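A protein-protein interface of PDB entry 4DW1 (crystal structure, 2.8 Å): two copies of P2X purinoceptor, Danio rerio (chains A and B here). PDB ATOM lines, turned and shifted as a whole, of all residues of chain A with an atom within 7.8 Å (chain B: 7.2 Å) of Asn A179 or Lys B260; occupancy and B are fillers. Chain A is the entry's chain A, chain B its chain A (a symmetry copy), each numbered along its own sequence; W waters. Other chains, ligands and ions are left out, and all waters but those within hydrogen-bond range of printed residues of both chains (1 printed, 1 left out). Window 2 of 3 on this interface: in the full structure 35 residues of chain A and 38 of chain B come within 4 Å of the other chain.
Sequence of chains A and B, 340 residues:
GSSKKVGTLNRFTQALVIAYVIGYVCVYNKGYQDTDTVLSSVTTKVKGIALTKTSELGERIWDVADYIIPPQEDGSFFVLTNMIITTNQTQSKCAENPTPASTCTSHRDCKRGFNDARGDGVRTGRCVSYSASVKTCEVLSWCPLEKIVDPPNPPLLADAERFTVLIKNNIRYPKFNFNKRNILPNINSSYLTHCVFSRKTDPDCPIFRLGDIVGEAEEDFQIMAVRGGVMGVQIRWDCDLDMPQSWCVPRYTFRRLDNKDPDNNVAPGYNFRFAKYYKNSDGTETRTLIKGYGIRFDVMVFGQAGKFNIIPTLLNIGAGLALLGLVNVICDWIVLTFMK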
ATOM      1  N   LEU A  39     -25.731 -15.106  20.737  1.00  0.00           N
ATOM      2  CA  LEU A  39     -25.224 -14.636  19.452  1.00  0.00           C
ATOM      3  C   LEU A  39     -24.066 -13.682  19.724  1.00  0.00           C
ATOM      4  O   LEU A  39     -24.190 -12.736  20.504  1.00  0.00           O
ATOM      5  CB  LEU A  39     -26.308 -13.945  18.628  1.00  0.00           C
ATOM      6  CG  LEU A  39     -27.570 -14.754  18.317  1.00  0.00           C
ATOM      7  CD1 LEU A  39     -28.508 -13.938  17.433  1.00  0.00           C
ATOM      8  CD2 LEU A  39     -27.250 -16.131  17.702  1.00  0.00           C
ATOM      9  N   SER A  41     -20.197 -11.653  18.524  1.00  0.00           N
ATOM     10  CA  SER A  41     -19.328 -11.061  17.519  1.00  0.00           C
ATOM     11  C   SER A  41     -18.048 -10.526  18.168  1.00  0.00           C
ATOM     12  O   SER A  41     -18.098  -9.899  19.221  1.00  0.00           O
ATOM     13  CB  SER A  41     -20.062  -9.939  16.795  1.00  0.00           C
ATOM     14  OG  SER A  41     -19.127  -9.099  16.149  1.00  0.00           O
ATOM     15  N   ASN A 169     -15.946  -7.968  22.467  1.00  0.00           N
ATOM     16  CA  ASN A 169     -16.941  -8.984  22.183  1.00  0.00           C
ATOM     17  C   ASN A 169     -18.377  -8.553  22.493  1.00  0.00           C
ATOM     18  O   ASN A 169     -18.747  -8.391  23.653  1.00  0.00           O
ATOM     19  CB  ASN A 169     -16.588 -10.220  22.996  1.00  0.00           C
ATOM     20  CG  ASN A 169     -17.611 -11.309  22.872  1.00  0.00           C
ATOM     21  OD1 ASN A 169     -17.840 -12.069  23.819  1.00  0.00           O
ATOM     22  ND2 ASN A 169     -18.234 -11.410  21.694  1.00  0.00           N
ATOM     23  N   ASN A 170     -19.189  -8.424  21.448  1.00  0.00           N
ATOM     24  CA  ASN A 170     -20.603  -8.114  21.587  1.00  0.00           C
ATOM     25  C   ASN A 170     -21.472  -9.358  21.577  1.00  0.00           C
ATOM     26  O   ASN A 170     -21.226 -10.286  20.829  1.00  0.00           O
ATOM     27  CB  ASN A 170     -21.033  -7.174  20.475  1.00  0.00           C
ATOM     28  CG  ASN A 170     -20.565  -5.748  20.710  1.00  0.00           C
ATOM     29  OD1 ASN A 170     -21.324  -4.904  21.190  1.00  0.00           O
ATOM     30  ND2 ASN A 170     -19.310  -5.473  20.378  1.00  0.00           N
ATOM     31  N   ILE A 171     -22.484  -9.390  22.426  1.00  0.00           N
ATOM     32  CA  ILE A 171     -23.360 -10.549  22.498  1.00  0.00           C
ATOM     33  C   ILE A 171     -24.791 -10.107  22.680  1.00  0.00           C
ATOM     34  O   ILE A 171     -25.062  -9.015  23.205  1.00  0.00           O
ATOM     35  CB  ILE A 171     -23.026 -11.454  23.678  1.00  0.00           C
ATOM     36  CG1 ILE A 171     -23.293 -10.703  24.991  1.00  0.00           C
ATOM     37  CG2 ILE A 171     -21.606 -11.955  23.569  1.00  0.00           C
ATOM     38  CD1 ILE A 171     -23.943 -11.543  26.054  1.00  0.00           C
ATOM     39  N   ARG A 172     -25.701 -10.971  22.239  1.00  0.00           N
ATOM     40  CA  ARG A 172     -27.125 -10.758  22.418  1.00  0.00           C
ATOM     41  C   ARG A 172     -27.804 -12.097  22.657  1.00  0.00           C
ATOM     42  O   ARG A 172     -27.330 -13.142  22.187  1.00  0.00           O
ATOM     43  CB  ARG A 172     -27.733 -10.049  21.206  1.00  0.00           C
ATOM     44  CG  ARG A 172     -28.766 -10.878  20.466  1.00  0.00           C
ATOM     45  CD  ARG A 172     -29.855 -10.018  19.824  1.00  0.00           C
ATOM     46  NE  ARG A 172     -30.450  -9.105  20.797  1.00  0.00           N
ATOM     47  CZ  ARG A 172     -31.611  -8.479  20.630  1.00  0.00           C
ATOM     48  NH1 ARG A 172     -32.320  -8.682  19.523  1.00  0.00           N
ATOM     49  NH2 ARG A 172     -32.064  -7.659  21.578  1.00  0.00           N
ATOM     50  N   TYR A 173     -28.901 -12.052  23.406  1.00  0.00           N
ATOM     51  CA  TYR A 173     -29.774 -13.203  23.630  1.00  0.00           C
ATOM     52  C   TYR A 173     -31.167 -12.808  23.163  1.00  0.00           C
ATOM     53  O   TYR A 173     -31.909 -12.149  23.896  1.00  0.00           O
ATOM     54  CB  TYR A 173     -29.816 -13.577  25.104  1.00  0.00           C
ATOM     55  CG  TYR A 173     -28.656 -14.418  25.566  1.00  0.00           C
ATOM     56  CD1 TYR A 173     -27.723 -13.920  26.461  1.00  0.00           C
ATOM     57  CD2 TYR A 173     -28.499 -15.712  25.111  1.00  0.00           C
ATOM     58  CE1 TYR A 173     -26.655 -14.696  26.887  1.00  0.00           C
ATOM     59  CE2 TYR A 173     -27.442 -16.494  25.533  1.00  0.00           C
ATOM     60  CZ  TYR A 173     -26.523 -15.982  26.417  1.00  0.00           C
ATOM     61  OH  TYR A 173     -25.483 -16.775  26.829  1.00  0.00           O
ATOM     62  N   PRO A 174     -31.502 -13.154  21.915  1.00  0.00           N
ATOM     63  CA  PRO A 174     -32.711 -12.629  21.260  1.00  0.00           C
ATOM     64  C   PRO A 174     -34.013 -12.872  22.030  1.00  0.00           C
ATOM     65  O   PRO A 174     -34.781 -11.924  22.210  1.00  0.00           O
ATOM     66  CB  PRO A 174     -32.727 -13.360  19.921  1.00  0.00           C
ATOM     67  CG  PRO A 174     -31.278 -13.709  19.680  1.00  0.00           C
ATOM     68  CD  PRO A 174     -30.719 -14.027  21.027  1.00  0.00           C
ATOM     69  N   PHE A 176     -34.508 -12.966  25.041  1.00  0.00           N
ATOM     70  CA  PHE A 176     -34.559 -12.073  26.181  1.00  0.00           C
ATOM     71  C   PHE A 176     -34.276 -10.618  25.822  1.00  0.00           C
ATOM     72  O   PHE A 176     -34.217  -9.764  26.705  1.00  0.00           O
ATOM     73  CB  PHE A 176     -33.617 -12.562  27.272  1.00  0.00           C
ATOM     74  CG  PHE A 176     -33.759 -14.028  27.575  1.00  0.00           C
ATOM     75  CD1 PHE A 176     -34.982 -14.556  27.948  1.00  0.00           C
ATOM     76  CD2 PHE A 176     -32.665 -14.879  27.495  1.00  0.00           C
ATOM     77  CE1 PHE A 176     -35.114 -15.910  28.237  1.00  0.00           C
ATOM     78  CE2 PHE A 176     -32.791 -16.238  27.783  1.00  0.00           C
ATOM     79  CZ  PHE A 176     -34.016 -16.752  28.155  1.00  0.00           C
ATOM     80  N   ASN A 177     -34.113 -10.334  24.531  1.00  0.00           N
ATOM     81  CA  ASN A 177     -33.793  -8.973  24.077  1.00  0.00           C
ATOM     82  C   ASN A 177     -32.639  -8.378  24.876  1.00  0.00           C
ATOM     83  O   ASN A 177     -32.597  -7.179  25.129  1.00  0.00           O
ATOM     84  CB  ASN A 177     -35.015  -8.049  24.161  1.00  0.00           C
ATOM     85  N   PHE A 178     -31.698  -9.234  25.254  1.00  0.00           N
ATOM     86  CA  PHE A 178     -30.614  -8.864  26.153  1.00  0.00           C
ATOM     87  C   PHE A 178     -29.292  -8.650  25.405  1.00  0.00           C
ATOM     88  O   PHE A 178     -28.754  -9.566  24.781  1.00  0.00           O
ATOM     89  CB  PHE A 178     -30.468  -9.932  27.236  1.00  0.00           C
ATOM     90  CG  PHE A 178     -29.280  -9.744  28.118  1.00  0.00           C
ATOM     91  CD1 PHE A 178     -29.356  -8.952  29.245  1.00  0.00           C
ATOM     92  CD2 PHE A 178     -28.081 -10.375  27.828  1.00  0.00           C
ATOM     93  CE1 PHE A 178     -28.258  -8.780  30.071  1.00  0.00           C
ATOM     94  CE2 PHE A 178     -26.977 -10.209  28.649  1.00  0.00           C
ATOM     95  CZ  PHE A 178     -27.065  -9.413  29.774  1.00  0.00           C
ATOM     96  N   ASN A 179     -28.789  -7.423  25.466  1.00  0.00           N
ATOM     97  CA  ASN A 179     -27.540  -7.057  24.816  1.00  0.00           C
ATOM     98  C   ASN A 179     -26.456  -6.781  25.834  1.00  0.00           C
ATOM     99  O   ASN A 179     -26.704  -6.158  26.872  1.00  0.00           O
ATOM    100  CB  ASN A 179     -27.736  -5.800  23.975  1.00  0.00           C
ATOM    101  CG  ASN A 179     -28.820  -5.963  22.951  1.00  0.00           C
ATOM    102  OD1 ASN A 179     -29.265  -7.079  22.678  1.00  0.00           O
ATOM    103  ND2 ASN A 179     -29.253  -4.853  22.368  1.00  0.00           N
ATOM    104  N   LYS A 180     -25.247  -7.235  25.547  1.00  0.00           N
ATOM    105  CA  LYS A 180     -24.127  -6.872  26.401  1.00  0.00           C
ATOM    106  C   LYS A 180     -22.815  -6.954  25.654  1.00  0.00           C
ATOM    107  O   LYS A 180     -22.747  -7.481  24.555  1.00  0.00           O
ATOM    108  CB  LYS A 180     -24.083  -7.707  27.674  1.00  0.00           C
ATOM    109  CG  LYS A 180     -23.837  -6.864  28.905  1.00  0.00           C
ATOM    110  CD  LYS A 180     -23.471  -7.703  30.111  1.00  0.00           C
ATOM    111  CE  LYS A 180     -23.189  -6.809  31.298  1.00  0.00           C
ATOM    112  NZ  LYS A 180     -22.949  -7.591  32.537  1.00  0.00           N
ATOM    113  N   ARG A 181     -21.778  -6.399  26.254  1.00  0.00           N
ATOM    114  CA  ARG A 181     -20.480  -6.311  25.627  1.00  0.00           C
ATOM    115  C   ARG A 181     -19.465  -6.653  26.707  1.00  0.00           C
ATOM    116  O   ARG A 181     -19.714  -6.399  27.878  1.00  0.00           O
ATOM    117  CB  ARG A 181     -20.305  -4.880  25.148  1.00  0.00           C
ATOM    118  CG  ARG A 181     -19.182  -4.623  24.217  1.00  0.00           C
ATOM    119  CD  ARG A 181     -19.466  -3.321  23.500  1.00  0.00           C
ATOM    120  NE  ARG A 181     -19.327  -2.177  24.384  1.00  0.00           N
ATOM    121  CZ  ARG A 181     -18.505  -1.165  24.141  1.00  0.00           C
ATOM    122  NH1 ARG A 181     -17.785  -1.171  23.029  1.00  0.00           N
ATOM    123  NH2 ARG A 181     -18.406  -0.153  24.992  1.00  0.00           N
ATOM    124  N   ASN A 182     -18.320  -7.211  26.334  1.00  0.00           N
ATOM    125  CA  ASN A 182     -17.354  -7.641  27.339  1.00  0.00           C
ATOM    126  C   ASN A 182     -16.503  -6.481  27.870  1.00  0.00           C
ATOM    127  O   ASN A 182     -15.616  -6.678  28.712  1.00  0.00           O
ATOM    128  CB  ASN A 182     -16.466  -8.769  26.827  1.00  0.00           C
ATOM    129  CG  ASN A 182     -15.359  -8.271  25.942  1.00  0.00           C
ATOM    130  OD1 ASN A 182     -15.511  -7.266  25.257  1.00  0.00           O
ATOM    131  ND2 ASN A 182     -14.233  -8.965  25.952  1.00  0.00           N
ATOM    132  N   TRP A 237     -20.295 -16.951  28.047  1.00  0.00           N
ATOM    133  CA  TRP A 237     -21.274 -16.085  28.701  1.00  0.00           C
ATOM    134  C   TRP A 237     -22.452 -16.938  29.170  1.00  0.00           C
ATOM    135  O   TRP A 237     -23.405 -17.143  28.432  1.00  0.00           O
ATOM    136  CB  TRP A 237     -21.836 -15.062  27.712  1.00  0.00           C
ATOM    137  CG  TRP A 237     -20.919 -13.957  27.240  1.00  0.00           C
ATOM    138  CD1 TRP A 237     -19.971 -14.036  26.255  1.00  0.00           C
ATOM    139  CD2 TRP A 237     -20.914 -12.587  27.686  1.00  0.00           C
ATOM    140  NE1 TRP A 237     -19.357 -12.811  26.084  1.00  0.00           N
ATOM    141  CE2 TRP A 237     -19.924 -11.906  26.944  1.00  0.00           C
ATOM    142  CE3 TRP A 237     -21.641 -11.874  28.650  1.00  0.00           C
ATOM    143  CZ2 TRP A 237     -19.644 -10.553  27.136  1.00  0.00           C
ATOM    144  CZ3 TRP A 237     -21.360 -10.529  28.837  1.00  0.00           C
ATOM    145  CH2 TRP A 237     -20.371  -9.884  28.087  1.00  0.00           C
ATOM    146  N   LEU A 241     -30.724 -14.973  33.998  1.00  0.00           N
ATOM    147  CA  LEU A 241     -31.259 -13.625  33.904  1.00  0.00           C
ATOM    148  C   LEU A 241     -32.266 -13.336  35.014  1.00  0.00           C
ATOM    149  O   LEU A 241     -32.796 -12.228  35.114  1.00  0.00           O
ATOM    150  CB  LEU A 241     -31.846 -13.359  32.515  1.00  0.00           C
ATOM    151  CG  LEU A 241     -30.776 -13.276  31.422  1.00  0.00           C
ATOM    152  CD1 LEU A 241     -31.360 -12.810  30.096  1.00  0.00           C
ATOM    153  CD2 LEU A 241     -29.655 -12.347  31.868  1.00  0.00           C
ATOM    154  N   GLN A 245     -28.532  -8.261  36.047  1.00  0.00           N
ATOM    155  CA  GLN A 245     -27.798  -8.215  34.791  1.00  0.00           C
ATOM    156  C   GLN A 245     -26.299  -7.946  35.022  1.00  0.00           C
ATOM    157  O   GLN A 245     -25.513  -7.957  34.081  1.00  0.00           O
ATOM    158  CB  GLN A 245     -28.407  -7.152  33.871  1.00  0.00           C
ATOM    159  N   CYS A 248     -23.815 -12.304  34.705  1.00  0.00           N
ATOM    160  CA  CYS A 248     -23.817 -12.289  33.255  1.00  0.00           C
ATOM    161  C   CYS A 248     -22.653 -11.382  32.907  1.00  0.00           C
ATOM    162  O   CYS A 248     -22.805 -10.223  32.497  1.00  0.00           O
ATOM    163  CB  CYS A 248     -25.125 -11.745  32.678  1.00  0.00           C
ATOM    164  SG  CYS A 248     -25.348 -12.203  30.943  1.00  0.00           S
ATOM    165  N   VAL B 230     -19.936  -3.296  12.845  1.00  0.00           N
ATOM    166  CA  VAL B 230     -20.182  -4.655  12.357  1.00  0.00           C
ATOM    167  C   VAL B 230     -21.649  -4.917  12.000  1.00  0.00           C
ATOM    168  O   VAL B 230     -22.531  -4.758  12.836  1.00  0.00           O
ATOM    169  CB  VAL B 230     -19.696  -5.728  13.373  1.00  0.00           C
ATOM    170  CG1 VAL B 230     -20.144  -7.113  12.952  1.00  0.00           C
ATOM    171  CG2 VAL B 230     -18.208  -5.687  13.477  1.00  0.00           C
ATOM    172  N   ARG B 255     -29.063  -7.031  10.704  1.00  0.00           N
ATOM    173  CA  ARG B 255     -28.968  -6.587  12.090  1.00  0.00           C
ATOM    174  C   ARG B 255     -27.604  -5.912  12.296  1.00  0.00           C
ATOM    175  O   ARG B 255     -26.662  -6.249  11.605  1.00  0.00           O
ATOM    176  CB  ARG B 255     -29.158  -7.793  13.025  1.00  0.00           C
ATOM    177  N   ARG B 256     -27.484  -4.941  13.197  1.00  0.00           N
ATOM    178  CA  ARG B 256     -26.147  -4.490  13.580  1.00  0.00           C
ATOM    179  C   ARG B 256     -25.629  -5.337  14.750  1.00  0.00           C
ATOM    180  O   ARG B 256     -26.318  -5.520  15.739  1.00  0.00           O
ATOM    181  CB  ARG B 256     -26.122  -3.018  13.950  1.00  0.00           C
ATOM    182  CG  ARG B 256     -24.813  -2.590  14.549  1.00  0.00           C
ATOM    183  CD  ARG B 256     -24.692  -1.087  14.642  1.00  0.00           C
ATOM    184  NE  ARG B 256     -23.322  -0.699  14.978  1.00  0.00           N
ATOM    185  CZ  ARG B 256     -22.882   0.555  15.073  1.00  0.00           C
ATOM    186  NH1 ARG B 256     -23.692   1.579  14.864  1.00  0.00           N
ATOM    187  NH2 ARG B 256     -21.614   0.783  15.364  1.00  0.00           N
ATOM    188  N   LEU B 257     -24.424  -5.879  14.601  1.00  0.00           N
ATOM    189  CA  LEU B 257     -23.852  -6.826  15.556  1.00  0.00           C
ATOM    190  C   LEU B 257     -23.166  -6.225  16.775  1.00  0.00           C
ATOM    191  O   LEU B 257     -23.257  -6.770  17.867  1.00  0.00           O
ATOM    192  CB  LEU B 257     -22.896  -7.763  14.837  1.00  0.00           C
ATOM    193  CG  LEU B 257     -23.654  -8.549  13.782  1.00  0.00           C
ATOM    194  CD1 LEU B 257     -22.751  -9.566  13.139  1.00  0.00           C
ATOM    195  CD2 LEU B 257     -24.840  -9.203  14.436  1.00  0.00           C
ATOM    196  N   ASP B 258     -22.451  -5.128  16.563  1.00  0.00           N
ATOM    197  CA  ASP B 258     -21.713  -4.439  17.612  1.00  0.00           C
ATOM    198  C   ASP B 258     -22.603  -3.405  18.281  1.00  0.00           C
ATOM    199  O   ASP B 258     -23.823  -3.412  18.106  1.00  0.00           O
ATOM    200  CB  ASP B 258     -20.484  -3.737  17.025  1.00  0.00           C
ATOM    201  CG  ASP B 258     -20.852  -2.694  15.994  1.00  0.00           C
ATOM    202  OD1 ASP B 258     -21.796  -2.937  15.227  1.00  0.00           O
ATOM    203  OD2 ASP B 258     -20.213  -1.630  15.937  1.00  0.00           O
ATOM    204  N   ASN B 259     -21.992  -2.524  19.064  1.00  0.00           N
ATOM    205  CA  ASN B 259     -22.730  -1.439  19.689  1.00  0.00           C
ATOM    206  C   ASN B 259     -23.802  -1.947  20.637  1.00  0.00           C
ATOM    207  O   ASN B 259     -24.913  -1.423  20.660  1.00  0.00           O
ATOM    208  CB  ASN B 259     -23.376  -0.549  18.627  1.00  0.00           C
ATOM    209  CG  ASN B 259     -23.907   0.751  19.212  1.00  0.00           C
ATOM    210  OD1 ASN B 259     -23.325   1.298  20.153  1.00  0.00           O
ATOM    211  ND2 ASN B 259     -25.027   1.243  18.671  1.00  0.00           N
ATOM    212  N   LYS B 260     -23.469  -2.971  21.415  1.00  0.00           N
ATOM    213  CA  LYS B 260     -24.436  -3.627  22.294  1.00  0.00           C
ATOM    214  C   LYS B 260     -24.482  -2.969  23.678  1.00  0.00           C
ATOM    215  O   LYS B 260     -25.184  -3.435  24.582  1.00  0.00           O
ATOM    216  CB  LYS B 260     -24.105  -5.115  22.435  1.00  0.00           C
ATOM    217  CG  LYS B 260     -24.209  -5.913  21.150  1.00  0.00           C
ATOM    218  CD  LYS B 260     -25.612  -6.483  20.942  1.00  0.00           C
ATOM    219  CE  LYS B 260     -26.488  -5.545  20.117  1.00  0.00           C
ATOM    220  NZ  LYS B 260     -26.079  -5.452  18.681  1.00  0.00           N
ATOM    221  N   ASP B 261     -23.707  -1.903  23.846  1.00  0.00           N
ATOM    222  CA  ASP B 261     -23.776  -1.092  25.055  1.00  0.00           C
ATOM    223  C   ASP B 261     -23.565   0.393  24.708  1.00  0.00           C
ATOM    224  O   ASP B 261     -22.570   1.005  25.117  1.00  0.00           O
ATOM    225  CB  ASP B 261     -22.760  -1.606  26.080  1.00  0.00           C
ATOM    226  CG  ASP B 261     -22.822  -0.865  27.406  1.00  0.00           C
ATOM    227  OD1 ASP B 261     -21.882  -1.064  28.208  1.00  0.00           O
ATOM    228  OD2 ASP B 261     -23.789  -0.099  27.647  1.00  0.00           O
ATOM    229  N   PRO B 262     -24.517   0.973  23.949  1.00  0.00           N
ATOM    230  CA  PRO B 262     -24.442   2.328  23.377  1.00  0.00           C
ATOM    231  C   PRO B 262     -24.284   3.468  24.386  1.00  0.00           C
ATOM    232  O   PRO B 262     -23.948   4.577  23.969  1.00  0.00           O
ATOM    233  CB  PRO B 262     -25.763   2.470  22.615  1.00  0.00           C
ATOM    234  CG  PRO B 262     -26.652   1.406  23.169  1.00  0.00           C
ATOM    235  CD  PRO B 262     -25.754   0.281  23.551  1.00  0.00           C
ATOM    236  N   ASP B 263     -24.536   3.220  25.670  1.00  0.00           N
ATOM    237  CA  ASP B 263     -24.292   4.235  26.700  1.00  0.00           C
ATOM    238  C   ASP B 263     -22.800   4.517  26.862  1.00  0.00           C
ATOM    239  O   ASP B 263     -22.417   5.568  27.372  1.00  0.00           O
ATOM    240  CB  ASP B 263     -24.859   3.802  28.054  1.00  0.00           C
ATOM    241  CG  ASP B 263     -26.255   3.249  27.948  1.00  0.00           C
ATOM    242  OD1 ASP B 263     -27.077   3.837  27.211  1.00  0.00           O
ATOM    243  OD2 ASP B 263     -26.523   2.216  28.597  1.00  0.00           O
ATOM    244  N   ASN B 264     -21.964   3.564  26.452  1.00  0.00           N
ATOM    245  CA  ASN B 264     -20.519   3.732  26.523  1.00  0.00           C
ATOM    246  C   ASN B 264     -19.986   4.643  25.431  1.00  0.00           C
ATOM    247  O   ASN B 264     -20.498   4.660  24.312  1.00  0.00           O
ATOM    248  CB  ASN B 264     -19.815   2.384  26.404  1.00  0.00           C
ATOM    249  CG  ASN B 264     -19.702   1.662  27.728  1.00  0.00           C
ATOM    250  OD1 ASN B 264     -19.875   0.437  27.799  1.00  0.00           O
ATOM    251  ND2 ASN B 264     -19.389   2.410  28.786  1.00  0.00           N
HETATM  252  O   HOH W   1     -23.130  -9.734  18.566  1.00  0.00           O
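The backbone NH (N) of Asn B259 lies within hydrogen-bond range of the side-chain amide oxygen (OD1) of Asn A170 (3.3 Å). The side-chain amide oxygen (OD1) of Asn A170 lies within hydrogen-bond range of the backbone NH (N) of Lys B260 (2.9 Å). The side-chain amide oxygen of Asn B264 is in hydrogen-bond range of the guanidinium group of Arg A181 (3.2 Å).
The backbone carbonyl oxygen of Lys A180 is in hydrogen-bond range of the backbone NH of Ile A171, at 2.9 Å. The backbone carbonyl oxygen (O) of Val B230 sits at hydrogen-bond distance from the backbone NH (N) of Leu B257, at 2.8 Å. The backbone carbonyl oxygen of Arg B256 sits at hydrogen-bond distance from the side-chain amino group of Lys B260, 3.0 Å away. The backbone carbonyl oxygen (O) of Leu B257 lies within hydrogen-bond range of the side-chain amino group (NZ) of Lys B260 (3.2 Å). The backbone carbonyl oxygen (O) of Asp B258 is in hydrogen-bond range of the side-chain amino group (NZ) of Lys B260 (3.1 Å). OD1 of Asn B264 sits close to OD1 of Asp B261 (2.5 Å).
Among the printed residues, merely in contact across the chains: Ser A41 with Val B230, Asn A170 with Leu B257, Asn A170 with Asp B258, Ile A171 with Lys B260, Asn A179 with Lys B260, Lys A180 with Lys B260 and Arg A181 with Asp B261.
Of the printed residues of chain B, Asn A179 touches Lys B260. Lys B260 touches just these residues of chain A: Asn A170 (2.9 Å), Ile A171 (3.4 Å), Asn A179 (3.5 Å) and Lys A180 (3.5 Å). Of the printed residues of chain B, Ile A171 touches Lys B260. Printed residues of chain B within 4 Å of Arg A181: Asp B261 and Asn B264. Of the printed residues of chain A, Leu B257 touches Asn A170. Of the printed residues of chain A, Asp B258 touches Asn A170 (3.5 Å). Of the printed residues of chain A, Val B230 touches Ser A41 (3.9 Å). Phe A176 touches none of the printed residues of chain B. Trp A237 touches none of the printed residues of chain B.
Of the 11 printed residues of chain B, 7 touch a printed residue of chain A. Among the printed residues, 10 pairs touch across the chains.
No position is printed for both chains. Of the 10 pairs that touch across the chains among the printed residues, none has its exchanged pair printed and touching as well.
Water W1 lies within hydrogen-bond range of O of Asn A170 and O of Leu B257.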
